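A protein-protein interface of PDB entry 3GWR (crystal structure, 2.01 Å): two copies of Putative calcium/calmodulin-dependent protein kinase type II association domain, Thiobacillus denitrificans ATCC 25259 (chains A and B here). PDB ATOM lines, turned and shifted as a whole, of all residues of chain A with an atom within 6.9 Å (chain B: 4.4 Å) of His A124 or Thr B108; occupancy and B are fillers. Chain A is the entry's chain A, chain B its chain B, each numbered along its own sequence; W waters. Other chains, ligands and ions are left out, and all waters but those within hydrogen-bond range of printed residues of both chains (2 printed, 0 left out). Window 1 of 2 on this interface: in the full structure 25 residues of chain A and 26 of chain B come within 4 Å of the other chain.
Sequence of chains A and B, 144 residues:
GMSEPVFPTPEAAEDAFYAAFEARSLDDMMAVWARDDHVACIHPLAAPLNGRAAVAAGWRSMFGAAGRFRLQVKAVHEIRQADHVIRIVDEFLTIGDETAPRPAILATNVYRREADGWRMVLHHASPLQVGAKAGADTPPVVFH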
ATOM      1  N   TRP A  33     -26.423  29.947   2.513  1.00  0.00           N
ATOM      2  CA  TRP A  33     -26.779  29.714   1.113  1.00  0.00           C
ATOM      3  C   TRP A  33     -27.329  30.939   0.393  1.00  0.00           C
ATOM      4  O   TRP A  33     -27.994  31.759   1.008  1.00  0.00           O
ATOM      5  CB  TRP A  33     -27.834  28.610   1.045  1.00  0.00           C
ATOM      6  CG  TRP A  33     -27.298  27.260   1.366  1.00  0.00           C
ATOM      7  CD1 TRP A  33     -27.068  26.727   2.608  1.00  0.00           C
ATOM      8  CD2 TRP A  33     -26.937  26.248   0.427  1.00  0.00           C
ATOM      9  NE1 TRP A  33     -26.597  25.445   2.498  1.00  0.00           N
ATOM     10  CE2 TRP A  33     -26.505  25.125   1.168  1.00  0.00           C
ATOM     11  CE3 TRP A  33     -26.929  26.182  -0.970  1.00  0.00           C
ATOM     12  CZ2 TRP A  33     -26.062  23.954   0.555  1.00  0.00           C
ATOM     13  CZ3 TRP A  33     -26.492  25.004  -1.581  1.00  0.00           C
ATOM     14  CH2 TRP A  33     -26.071  23.915  -0.822  1.00  0.00           C
ATOM     15  N   ALA A  40     -28.013  24.014  -5.230  1.00  0.00           N
ATOM     16  CA  ALA A  40     -28.234  22.550  -5.184  1.00  0.00           C
ATOM     17  C   ALA A  40     -27.355  21.934  -4.111  1.00  0.00           C
ATOM     18  O   ALA A  40     -26.342  22.518  -3.722  1.00  0.00           O
ATOM     19  CB  ALA A  40     -27.959  21.908  -6.547  1.00  0.00           C
ATOM     20  N   CYS A  41     -27.740  20.763  -3.626  1.00  0.00           N
ATOM     21  CA  CYS A  41     -26.995  20.109  -2.556  1.00  0.00           C
ATOM     22  C   CYS A  41     -27.100  18.619  -2.741  1.00  0.00           C
ATOM     23  O   CYS A  41     -28.231  18.086  -2.889  1.00  0.00           O
ATOM     24  CB  CYS A  41     -27.589  20.536  -1.231  1.00  0.00           C
ATOM     25  SG  CYS A  41     -26.686  19.997   0.219  1.00  0.00           S
ATOM     26  N   ILE A  42     -25.943  17.948  -2.748  1.00  0.00           N
ATOM     27  CA  ILE A  42     -25.864  16.482  -2.919  1.00  0.00           C
ATOM     28  C   ILE A  42     -25.235  15.916  -1.652  1.00  0.00           C
ATOM     29  O   ILE A  42     -24.090  16.227  -1.354  1.00  0.00           O
ATOM     30  CB  ILE A  42     -25.013  16.091  -4.178  1.00  0.00           C
ATOM     31  CG1 ILE A  42     -25.657  16.653  -5.457  1.00  0.00           C
ATOM     32  CG2 ILE A  42     -24.891  14.579  -4.340  1.00  0.00           C
ATOM     33  CD1 ILE A  42     -24.601  16.964  -6.572  1.00  0.00           C
ATOM     34  N   HIS A  43     -26.015  15.151  -0.894  1.00  0.00           N
ATOM     35  CA  HIS A  43     -25.545  14.470   0.321  1.00  0.00           C
ATOM     36  C   HIS A  43     -24.928  13.139  -0.123  1.00  0.00           C
ATOM     37  O   HIS A  43     -25.191  12.670  -1.214  1.00  0.00           O
ATOM     38  CB  HIS A  43     -26.671  14.279   1.352  1.00  0.00           C
ATOM     39  CG  HIS A  43     -27.185  15.570   1.926  1.00  0.00           C
ATOM     40  ND1 HIS A  43     -26.410  16.403   2.702  1.00  0.00           N
ATOM     41  CD2 HIS A  43     -28.392  16.173   1.825  1.00  0.00           C
ATOM     42  CE1 HIS A  43     -27.111  17.470   3.037  1.00  0.00           C
ATOM     43  NE2 HIS A  43     -28.317  17.356   2.517  1.00  0.00           N
ATOM     44  N   PRO A  44     -24.098  12.520   0.728  1.00  0.00           N
ATOM     45  CA  PRO A  44     -23.421  11.320   0.282  1.00  0.00           C
ATOM     46  C   PRO A  44     -24.333  10.254  -0.276  1.00  0.00           C
ATOM     47  O   PRO A  44     -25.267   9.833   0.384  1.00  0.00           O
ATOM     48  CB  PRO A  44     -22.684  10.849   1.522  1.00  0.00           C
ATOM     49  CG  PRO A  44     -22.421  12.114   2.276  1.00  0.00           C
ATOM     50  CD  PRO A  44     -23.651  12.943   2.067  1.00  0.00           C
ATOM     51  N   ALA A  46     -26.529  10.440  -2.485  1.00  0.00           N
ATOM     52  CA  ALA A  46     -27.871  10.913  -2.821  1.00  0.00           C
ATOM     53  C   ALA A  46     -27.933  11.601  -4.188  1.00  0.00           C
ATOM     54  O   ALA A  46     -26.896  11.936  -4.797  1.00  0.00           O
ATOM     55  CB  ALA A  46     -28.373  11.834  -1.724  1.00  0.00           C
ATOM     56  N   GLU A  91     -14.003  15.984   5.162  1.00  0.00           N
ATOM     57  CA  GLU A  91     -14.855  16.145   6.335  1.00  0.00           C
ATOM     58  C   GLU A  91     -14.745  14.893   7.230  1.00  0.00           C
ATOM     59  O   GLU A  91     -15.037  13.768   6.796  1.00  0.00           O
ATOM     60  CB  GLU A  91     -16.330  16.321   5.930  1.00  0.00           C
ATOM     61  CG  GLU A  91     -16.636  17.386   4.923  1.00  0.00           C
ATOM     62  CD  GLU A  91     -18.113  17.432   4.539  1.00  0.00           C
ATOM     63  OE1 GLU A  91     -18.855  16.402   4.720  1.00  0.00           O
ATOM     64  OE2 GLU A  91     -18.541  18.513   4.065  1.00  0.00           O
ATOM     65  N   ILE A 105     -15.425  12.014   4.340  1.00  0.00           N
ATOM     66  CA  ILE A 105     -16.380  12.311   3.296  1.00  0.00           C
ATOM     67  C   ILE A 105     -15.692  13.449   2.547  1.00  0.00           C
ATOM     68  O   ILE A 105     -15.107  14.340   3.169  1.00  0.00           O
ATOM     69  CB  ILE A 105     -17.735  12.765   3.858  1.00  0.00           C
ATOM     70  CG1 ILE A 105     -18.444  11.626   4.601  1.00  0.00           C
ATOM     71  CG2 ILE A 105     -18.633  13.303   2.744  1.00  0.00           C
ATOM     72  CD1 ILE A 105     -18.780  10.413   3.756  1.00  0.00           C
ATOM     73  N   LEU A 106     -15.716  13.405   1.219  1.00  0.00           N
ATOM     74  CA  LEU A 106     -15.096  14.441   0.428  1.00  0.00           C
ATOM     75  C   LEU A 106     -16.204  15.385   0.027  1.00  0.00           C
ATOM     76  O   LEU A 106     -17.287  14.918  -0.338  1.00  0.00           O
ATOM     77  CB  LEU A 106     -14.461  13.843  -0.822  1.00  0.00           C
ATOM     78  CG  LEU A 106     -13.790  14.806  -1.808  1.00  0.00           C
ATOM     79  CD1 LEU A 106     -12.513  15.334  -1.217  1.00  0.00           C
ATOM     80  CD2 LEU A 106     -13.499  14.099  -3.171  1.00  0.00           C
ATOM     81  N   ALA A 107     -15.954  16.697   0.062  1.00  0.00           N
ATOM     82  CA  ALA A 107     -16.988  17.647  -0.346  1.00  0.00           C
ATOM     83  C   ALA A 107     -16.486  18.750  -1.270  1.00  0.00           C
ATOM     84  O   ALA A 107     -15.441  19.345  -1.035  1.00  0.00           O
ATOM     85  CB  ALA A 107     -17.639  18.271   0.890  1.00  0.00           C
ATOM     86  N   THR A 108     -17.223  19.002  -2.332  1.00  0.00           N
ATOM     87  CA  THR A 108     -16.979  20.174  -3.168  1.00  0.00           C
ATOM     88  C   THR A 108     -17.973  21.275  -2.758  1.00  0.00           C
ATOM     89  O   THR A 108     -19.160  21.104  -2.879  1.00  0.00           O
ATOM     90  CB  THR A 108     -17.115  19.844  -4.677  1.00  0.00           C
ATOM     91  OG1 THR A 108     -16.077  18.909  -5.031  1.00  0.00           O
ATOM     92  CG2 THR A 108     -16.957  21.105  -5.520  1.00  0.00           C
ATOM     93  N   ASN A 109     -17.466  22.418  -2.305  1.00  0.00           N
ATOM     94  CA  ASN A 109     -18.298  23.584  -1.973  1.00  0.00           C
ATOM     95  C   ASN A 109     -17.993  24.741  -2.946  1.00  0.00           C
ATOM     96  O   ASN A 109     -16.824  25.061  -3.177  1.00  0.00           O
ATOM     97  CB  ASN A 109     -17.975  24.011  -0.513  1.00  0.00           C
ATOM     98  CG  ASN A 109     -18.244  22.900   0.510  1.00  0.00           C
ATOM     99  OD1 ASN A 109     -19.218  22.135   0.390  1.00  0.00           O
ATOM    100  ND2 ASN A 109     -17.400  22.827   1.537  1.00  0.00           N
ATOM    101  N   VAL A 110     -19.031  25.402  -3.453  1.00  0.00           N
ATOM    102  CA  VAL A 110     -18.909  26.476  -4.407  1.00  0.00           C
ATOM    103  C   VAL A 110     -19.587  27.724  -3.852  1.00  0.00           C
ATOM    104  O   VAL A 110     -20.768  27.695  -3.497  1.00  0.00           O
ATOM    105  CB  VAL A 110     -19.519  26.090  -5.785  1.00  0.00           C
ATOM    106  CG1 VAL A 110     -19.318  27.232  -6.836  1.00  0.00           C
ATOM    107  CG2 VAL A 110     -18.884  24.756  -6.277  1.00  0.00           C
ATOM    108  N   LEU A 122     -23.516  25.591  -4.021  1.00  0.00           N
ATOM    109  CA  LEU A 122     -23.504  24.125  -4.158  1.00  0.00           C
ATOM    110  C   LEU A 122     -22.649  23.430  -3.114  1.00  0.00           C
ATOM    111  O   LEU A 122     -21.566  23.909  -2.761  1.00  0.00           O
ATOM    112  CB  LEU A 122     -22.911  23.734  -5.526  1.00  0.00           C
ATOM    113  CG  LEU A 122     -22.905  22.237  -5.925  1.00  0.00           C
ATOM    114  CD1 LEU A 122     -23.969  21.942  -6.953  1.00  0.00           C
ATOM    115  CD2 LEU A 122     -21.576  21.844  -6.513  1.00  0.00           C
ATOM    116  N   HIS A 123     -23.107  22.243  -2.715  1.00  0.00           N
ATOM    117  CA  HIS A 123     -22.384  21.329  -1.819  1.00  0.00           C
ATOM    118  C   HIS A 123     -22.568  19.975  -2.430  1.00  0.00           C
ATOM    119  O   HIS A 123     -23.693  19.583  -2.660  1.00  0.00           O
ATOM    120  CB  HIS A 123     -23.003  21.341  -0.428  1.00  0.00           C
ATOM    121  CG  HIS A 123     -22.414  20.348   0.533  1.00  0.00           C
ATOM    122  ND1 HIS A 123     -21.156  20.493   1.074  1.00  0.00           N
ATOM    123  CD2 HIS A 123     -22.948  19.233   1.102  1.00  0.00           C
ATOM    124  CE1 HIS A 123     -20.918  19.486   1.894  1.00  0.00           C
ATOM    125  NE2 HIS A 123     -21.994  18.717   1.947  1.00  0.00           N
ATOM    126  N   HIS A 124     -21.473  19.278  -2.711  1.00  0.00           N
ATOM    127  CA  HIS A 124     -21.521  17.942  -3.294  1.00  0.00           C
ATOM    128  C   HIS A 124     -20.583  17.076  -2.462  1.00  0.00           C
ATOM    129  O   HIS A 124     -19.345  17.247  -2.502  1.00  0.00           O
ATOM    130  CB  HIS A 124     -21.068  17.989  -4.764  1.00  0.00           C
ATOM    131  CG  HIS A 124     -21.209  16.694  -5.496  1.00  0.00           C
ATOM    132  ND1 HIS A 124     -21.223  16.624  -6.874  1.00  0.00           N
ATOM    133  CD2 HIS A 124     -21.354  15.423  -5.050  1.00  0.00           C
ATOM    134  CE1 HIS A 124     -21.383  15.358  -7.245  1.00  0.00           C
ATOM    135  NE2 HIS A 124     -21.457  14.608  -6.159  1.00  0.00           N
ATOM    136  N   ALA A 125     -21.181  16.184  -1.676  1.00  0.00           N
ATOM    137  CA  ALA A 125     -20.443  15.297  -0.768  1.00  0.00           C
ATOM    138  C   ALA A 125     -20.448  13.878  -1.277  1.00  0.00           C
ATOM    139  O   ALA A 125     -21.475  13.391  -1.783  1.00  0.00           O
ATOM    140  CB  ALA A 125     -21.046  15.359   0.660  1.00  0.00           C
ATOM    141  N   SER A 126     -19.302  13.213  -1.164  1.00  0.00           N
ATOM    142  CA  SER A 126     -19.193  11.822  -1.590  1.00  0.00           C
ATOM    143  C   SER A 126     -18.239  11.051  -0.703  1.00  0.00           C
ATOM    144  O   SER A 126     -17.359  11.648  -0.095  1.00  0.00           O
ATOM    145  CB  SER A 126     -18.718  11.725  -3.023  1.00  0.00           C
ATOM    146  OG  SER A 126     -17.453  12.344  -3.204  1.00  0.00           O
ATOM    147  N   ILE B  86     -22.806  25.451 -13.791  1.00  0.00           N
ATOM    148  CA  ILE B  86     -22.720  24.127 -13.179  1.00  0.00           C
ATOM    149  C   ILE B  86     -23.835  23.275 -13.757  1.00  0.00           C
ATOM    150  O   ILE B  86     -24.979  23.714 -13.783  1.00  0.00           O
ATOM    151  CB  ILE B  86     -22.904  24.208 -11.658  1.00  0.00           C
ATOM    152  CG1 ILE B  86     -21.833  25.127 -11.072  1.00  0.00           C
ATOM    153  CG2 ILE B  86     -22.839  22.796 -11.069  1.00  0.00           C
ATOM    154  CD1 ILE B  86     -22.122  25.538  -9.592  1.00  0.00           C
ATOM    155  N   ARG B  87     -23.485  22.110 -14.294  1.00  0.00           N
ATOM    156  CA  ARG B  87     -24.446  21.161 -14.850  1.00  0.00           C
ATOM    157  C   ARG B  87     -24.338  19.864 -14.081  1.00  0.00           C
ATOM    158  O   ARG B  87     -23.241  19.338 -13.906  1.00  0.00           O
ATOM    159  CB  ARG B  87     -24.201  20.960 -16.351  1.00  0.00           C
ATOM    160  CG  ARG B  87     -24.561  22.244 -17.124  1.00  0.00           C
ATOM    161  CD  ARG B  87     -24.390  22.149 -18.607  1.00  0.00           C
ATOM    162  NE  ARG B  87     -25.301  21.176 -19.209  1.00  0.00           N
ATOM    163  CZ  ARG B  87     -26.508  21.434 -19.692  1.00  0.00           C
ATOM    164  NH1 ARG B  87     -27.077  22.624 -19.589  1.00  0.00           N
ATOM    165  NH2 ARG B  87     -27.173  20.444 -20.250  1.00  0.00           N
ATOM    166  N   ILE B  88     -25.465  19.413 -13.527  1.00  0.00           N
ATOM    167  CA  ILE B  88     -25.546  18.159 -12.780  1.00  0.00           C
ATOM    168  C   ILE B  88     -26.222  17.152 -13.689  1.00  0.00           C
ATOM    169  O   ILE B  88     -27.345  17.407 -14.163  1.00  0.00           O
ATOM    170  CB  ILE B  88     -26.295  18.331 -11.435  1.00  0.00           C
ATOM    171  CG1 ILE B  88     -25.605  19.423 -10.598  1.00  0.00           C
ATOM    172  CG2 ILE B  88     -26.336  17.007 -10.677  1.00  0.00           C
ATOM    173  CD1 ILE B  88     -26.378  19.871  -9.357  1.00  0.00           C
ATOM    174  N   ALA B 107     -22.851  13.298 -11.677  1.00  0.00           N
ATOM    175  CA  ALA B 107     -21.688  14.135 -11.844  1.00  0.00           C
ATOM    176  C   ALA B 107     -22.055  15.603 -11.829  1.00  0.00           C
ATOM    177  O   ALA B 107     -23.040  16.023 -12.439  1.00  0.00           O
ATOM    178  CB  ALA B 107     -20.930  13.787 -13.149  1.00  0.00           C
ATOM    179  N   THR B 108     -21.269  16.362 -11.092  1.00  0.00           N
ATOM    180  CA  THR B 108     -21.322  17.804 -11.125  1.00  0.00           C
ATOM    181  C   THR B 108     -20.165  18.254 -12.017  1.00  0.00           C
ATOM    182  O   THR B 108     -18.987  17.973 -11.706  1.00  0.00           O
ATOM    183  CB  THR B 108     -21.116  18.376  -9.730  1.00  0.00           C
ATOM    184  OG1 THR B 108     -22.217  17.963  -8.907  1.00  0.00           O
ATOM    185  CG2 THR B 108     -21.025  19.888  -9.796  1.00  0.00           C
ATOM    186  N   ASN B 109     -20.488  18.957 -13.105  1.00  0.00           N
ATOM    187  CA  ASN B 109     -19.514  19.496 -14.042  1.00  0.00           C
ATOM    188  C   ASN B 109     -19.584  21.031 -14.022  1.00  0.00           C
ATOM    189  O   ASN B 109     -20.670  21.630 -14.120  1.00  0.00           O
ATOM    190  CB  ASN B 109     -19.784  18.966 -15.462  1.00  0.00           C
ATOM    191  CG  ASN B 109     -19.659  17.455 -15.579  1.00  0.00           C
ATOM    192  OD1 ASN B 109     -18.721  16.840 -15.020  1.00  0.00           O
ATOM    193  ND2 ASN B 109     -20.567  16.831 -16.381  1.00  0.00           N
ATOM    194  N   VAL B 110     -18.451  21.667 -13.809  1.00  0.00           N
ATOM    195  CA  VAL B 110     -18.381  23.115 -13.698  1.00  0.00           C
ATOM    196  C   VAL B 110     -17.590  23.658 -14.876  1.00  0.00           C
ATOM    197  O   VAL B 110     -16.437  23.249 -15.084  1.00  0.00           O
ATOM    198  CB  VAL B 110     -17.673  23.565 -12.381  1.00  0.00           C
ATOM    199  CG1 VAL B 110     -17.619  25.088 -12.320  1.00  0.00           C
ATOM    200  CG2 VAL B 110     -18.362  22.958 -11.121  1.00  0.00           C
ATOM    201  N   LEU B 122     -13.877  21.630 -13.263  1.00  0.00           N
ATOM    202  CA  LEU B 122     -14.111  20.588 -12.253  1.00  0.00           C
ATOM    203  C   LEU B 122     -15.130  19.565 -12.737  1.00  0.00           C
ATOM    204  O   LEU B 122     -16.101  19.927 -13.374  1.00  0.00           O
ATOM    205  CB  LEU B 122     -14.681  21.190 -10.971  1.00  0.00           C
ATOM    206  CG  LEU B 122     -14.958  20.196  -9.799  1.00  0.00           C
ATOM    207  CD1 LEU B 122     -13.885  20.307  -8.772  1.00  0.00           C
ATOM    208  CD2 LEU B 122     -16.284  20.479  -9.117  1.00  0.00           C
ATOM    209  N   HIS B 123     -14.879  18.303 -12.402  1.00  0.00           N
ATOM    210  CA  HIS B 123     -15.761  17.163 -12.643  1.00  0.00           C
ATOM    211  C   HIS B 123     -15.761  16.441 -11.315  1.00  0.00           C
ATOM    212  O   HIS B 123     -14.688  16.105 -10.799  1.00  0.00           O
ATOM    213  CB  HIS B 123     -15.185  16.278 -13.751  1.00  0.00           C
ATOM    214  CG  HIS B 123     -15.897  14.975 -13.935  1.00  0.00           C
ATOM    215  ND1 HIS B 123     -17.160  14.887 -14.477  1.00  0.00           N
ATOM    216  CD2 HIS B 123     -15.512  13.694 -13.668  1.00  0.00           C
ATOM    217  CE1 HIS B 123     -17.523  13.612 -14.553  1.00  0.00           C
ATOM    218  NE2 HIS B 123     -16.543  12.866 -14.061  1.00  0.00           N
ATOM    219  N   HIS B 124     -16.940  16.281 -10.711  1.00  0.00           N
ATOM    220  CA  HIS B 124     -17.090  15.565  -9.424  1.00  0.00           C
ATOM    221  C   HIS B 124     -18.159  14.516  -9.660  1.00  0.00           C
ATOM    222  O   HIS B 124     -19.354  14.847  -9.714  1.00  0.00           O
ATOM    223  CB  HIS B 124     -17.508  16.512  -8.290  1.00  0.00           C
ATOM    224  CG  HIS B 124     -17.489  15.905  -6.909  1.00  0.00           C
ATOM    225  ND1 HIS B 124     -17.322  16.670  -5.767  1.00  0.00           N
ATOM    226  CD2 HIS B 124     -17.638  14.624  -6.481  1.00  0.00           C
ATOM    227  CE1 HIS B 124     -17.367  15.885  -4.703  1.00  0.00           C
ATOM    228  NE2 HIS B 124     -17.576  14.638  -5.108  1.00  0.00           N
ATOM    229  N   SER B 126     -20.007  10.793  -8.483  1.00  0.00           N
ATOM    230  CA  SER B 126     -20.345  10.050  -7.269  1.00  0.00           C
ATOM    231  C   SER B 126     -21.427   9.007  -7.538  1.00  0.00           C
ATOM    232  O   SER B 126     -22.288   9.210  -8.397  1.00  0.00           O
ATOM    233  CB  SER B 126     -20.791  11.020  -6.145  1.00  0.00           C
ATOM    234  OG  SER B 126     -21.912  11.831  -6.500  1.00  0.00           O
HETATM  235  O   HOH W   1     -22.282  11.311  -3.214  1.00  0.00           O
HETATM  236  O   HOH W   2     -24.157  10.950  -5.183  1.00  0.00           O
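Of chain B, only Thr B108 (2.6 Å), His B124 (3.2 Å) and Ser B126 (2.8 Å) come within 4 Å of His A124. Of the printed residues of chain B, Thr A108 touches Leu B122 (3.7 Å) and His B124 (2.7 Å). Of the printed residues of chain B, Ala A40 touches Ile B88.
The side-chain hydroxyl (OG1) of Thr B108 sits at hydrogen-bond distance from a ring nitrogen (ND1) of His A124 (2.6 Å). The side-chain hydroxyl of Thr A108 lies within hydrogen-bond range of a ring nitrogen (ND1) of His B124 (2.7 Å). The side-chain hydroxyl (OG) of Ser B126 is in hydrogen-bond range of a ring nitrogen (NE2) of His A124 (2.8 Å). OG of Ser A126 lies within hydrogen-bond range of NE2 of His B124.
Thr A108 touches Leu B122, and with the chains exchanged Leu A122 touches Thr B108. Thr A108 touches His B124, and with the chains exchanged His A124 touches Thr B108. His B124 touches its own counterpart, His A124. Ser A126 touches its own counterpart, Ser B126.
O of Ala A40 lies within hydrogen-bond range of N of His A123, at 3.4 Å. O of Ile A42 sits at hydrogen-bond distance from N of Ala A125 (2.9 Å). The backbone carbonyl oxygen (O) of Ser A126 lies within hydrogen-bond range of the backbone NH (N) of Leu A106. The backbone NH (N) of Ile A42 sits at hydrogen-bond distance from the backbone carbonyl oxygen (O) of His A123 (2.8 Å). N of Val B110 lies within hydrogen-bond range of O of Leu B122 (3.0 Å). The backbone carbonyl oxygen of His A124 lies within hydrogen-bond range of the backbone NH of Thr A108 (2.8 Å).
Ala A40 touches Ile B88 (CB to CD1, 3.8 Å). CD1 of Ile A42 touches OG1 of Thr B108 (3.5 Å). CD2 of Leu B122 touches CG2 of Thr A108 (3.7 Å). Leu A122 touches Ile B88. CG2 of Thr B108 touches CD2 of Leu A122, 3.9 Å away. His B124 touches His A124. CB of Ser A126 touches CB of Ser B126, 3.8 Å away.
Of the 11 printed residues of chain B, 5 touch a printed residue of chain A. Printed residues of chain B that touch a printed residue of chain A: Ile B88, Thr B108, Leu B122, His B124 and Ser B126. Of the 19 printed residues of chain A, 6 touch a printed residue of chain B. Hydrophobic or aromatic side chains of chain A that line the printed part of chain B: Ala A40, Ile A42, Leu A122 and His A124. Among the printed residues, 11 pairs touch across the chains. Among the printed residues, no Asp or Glu carboxylate lies within 4 Å of a Lys or Arg side-chain nitrogen of the other chain.
Water W1 bridges the backbone carbonyl oxygen of Ala A125 (2.7 Å) and the side-chain hydroxyl of Ser B126 (3.3 Å). Water W2 lies within hydrogen-bond range of the side-chain hydroxyl of Ser B126 and the backbone carbonyl oxygen of Ala A46.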
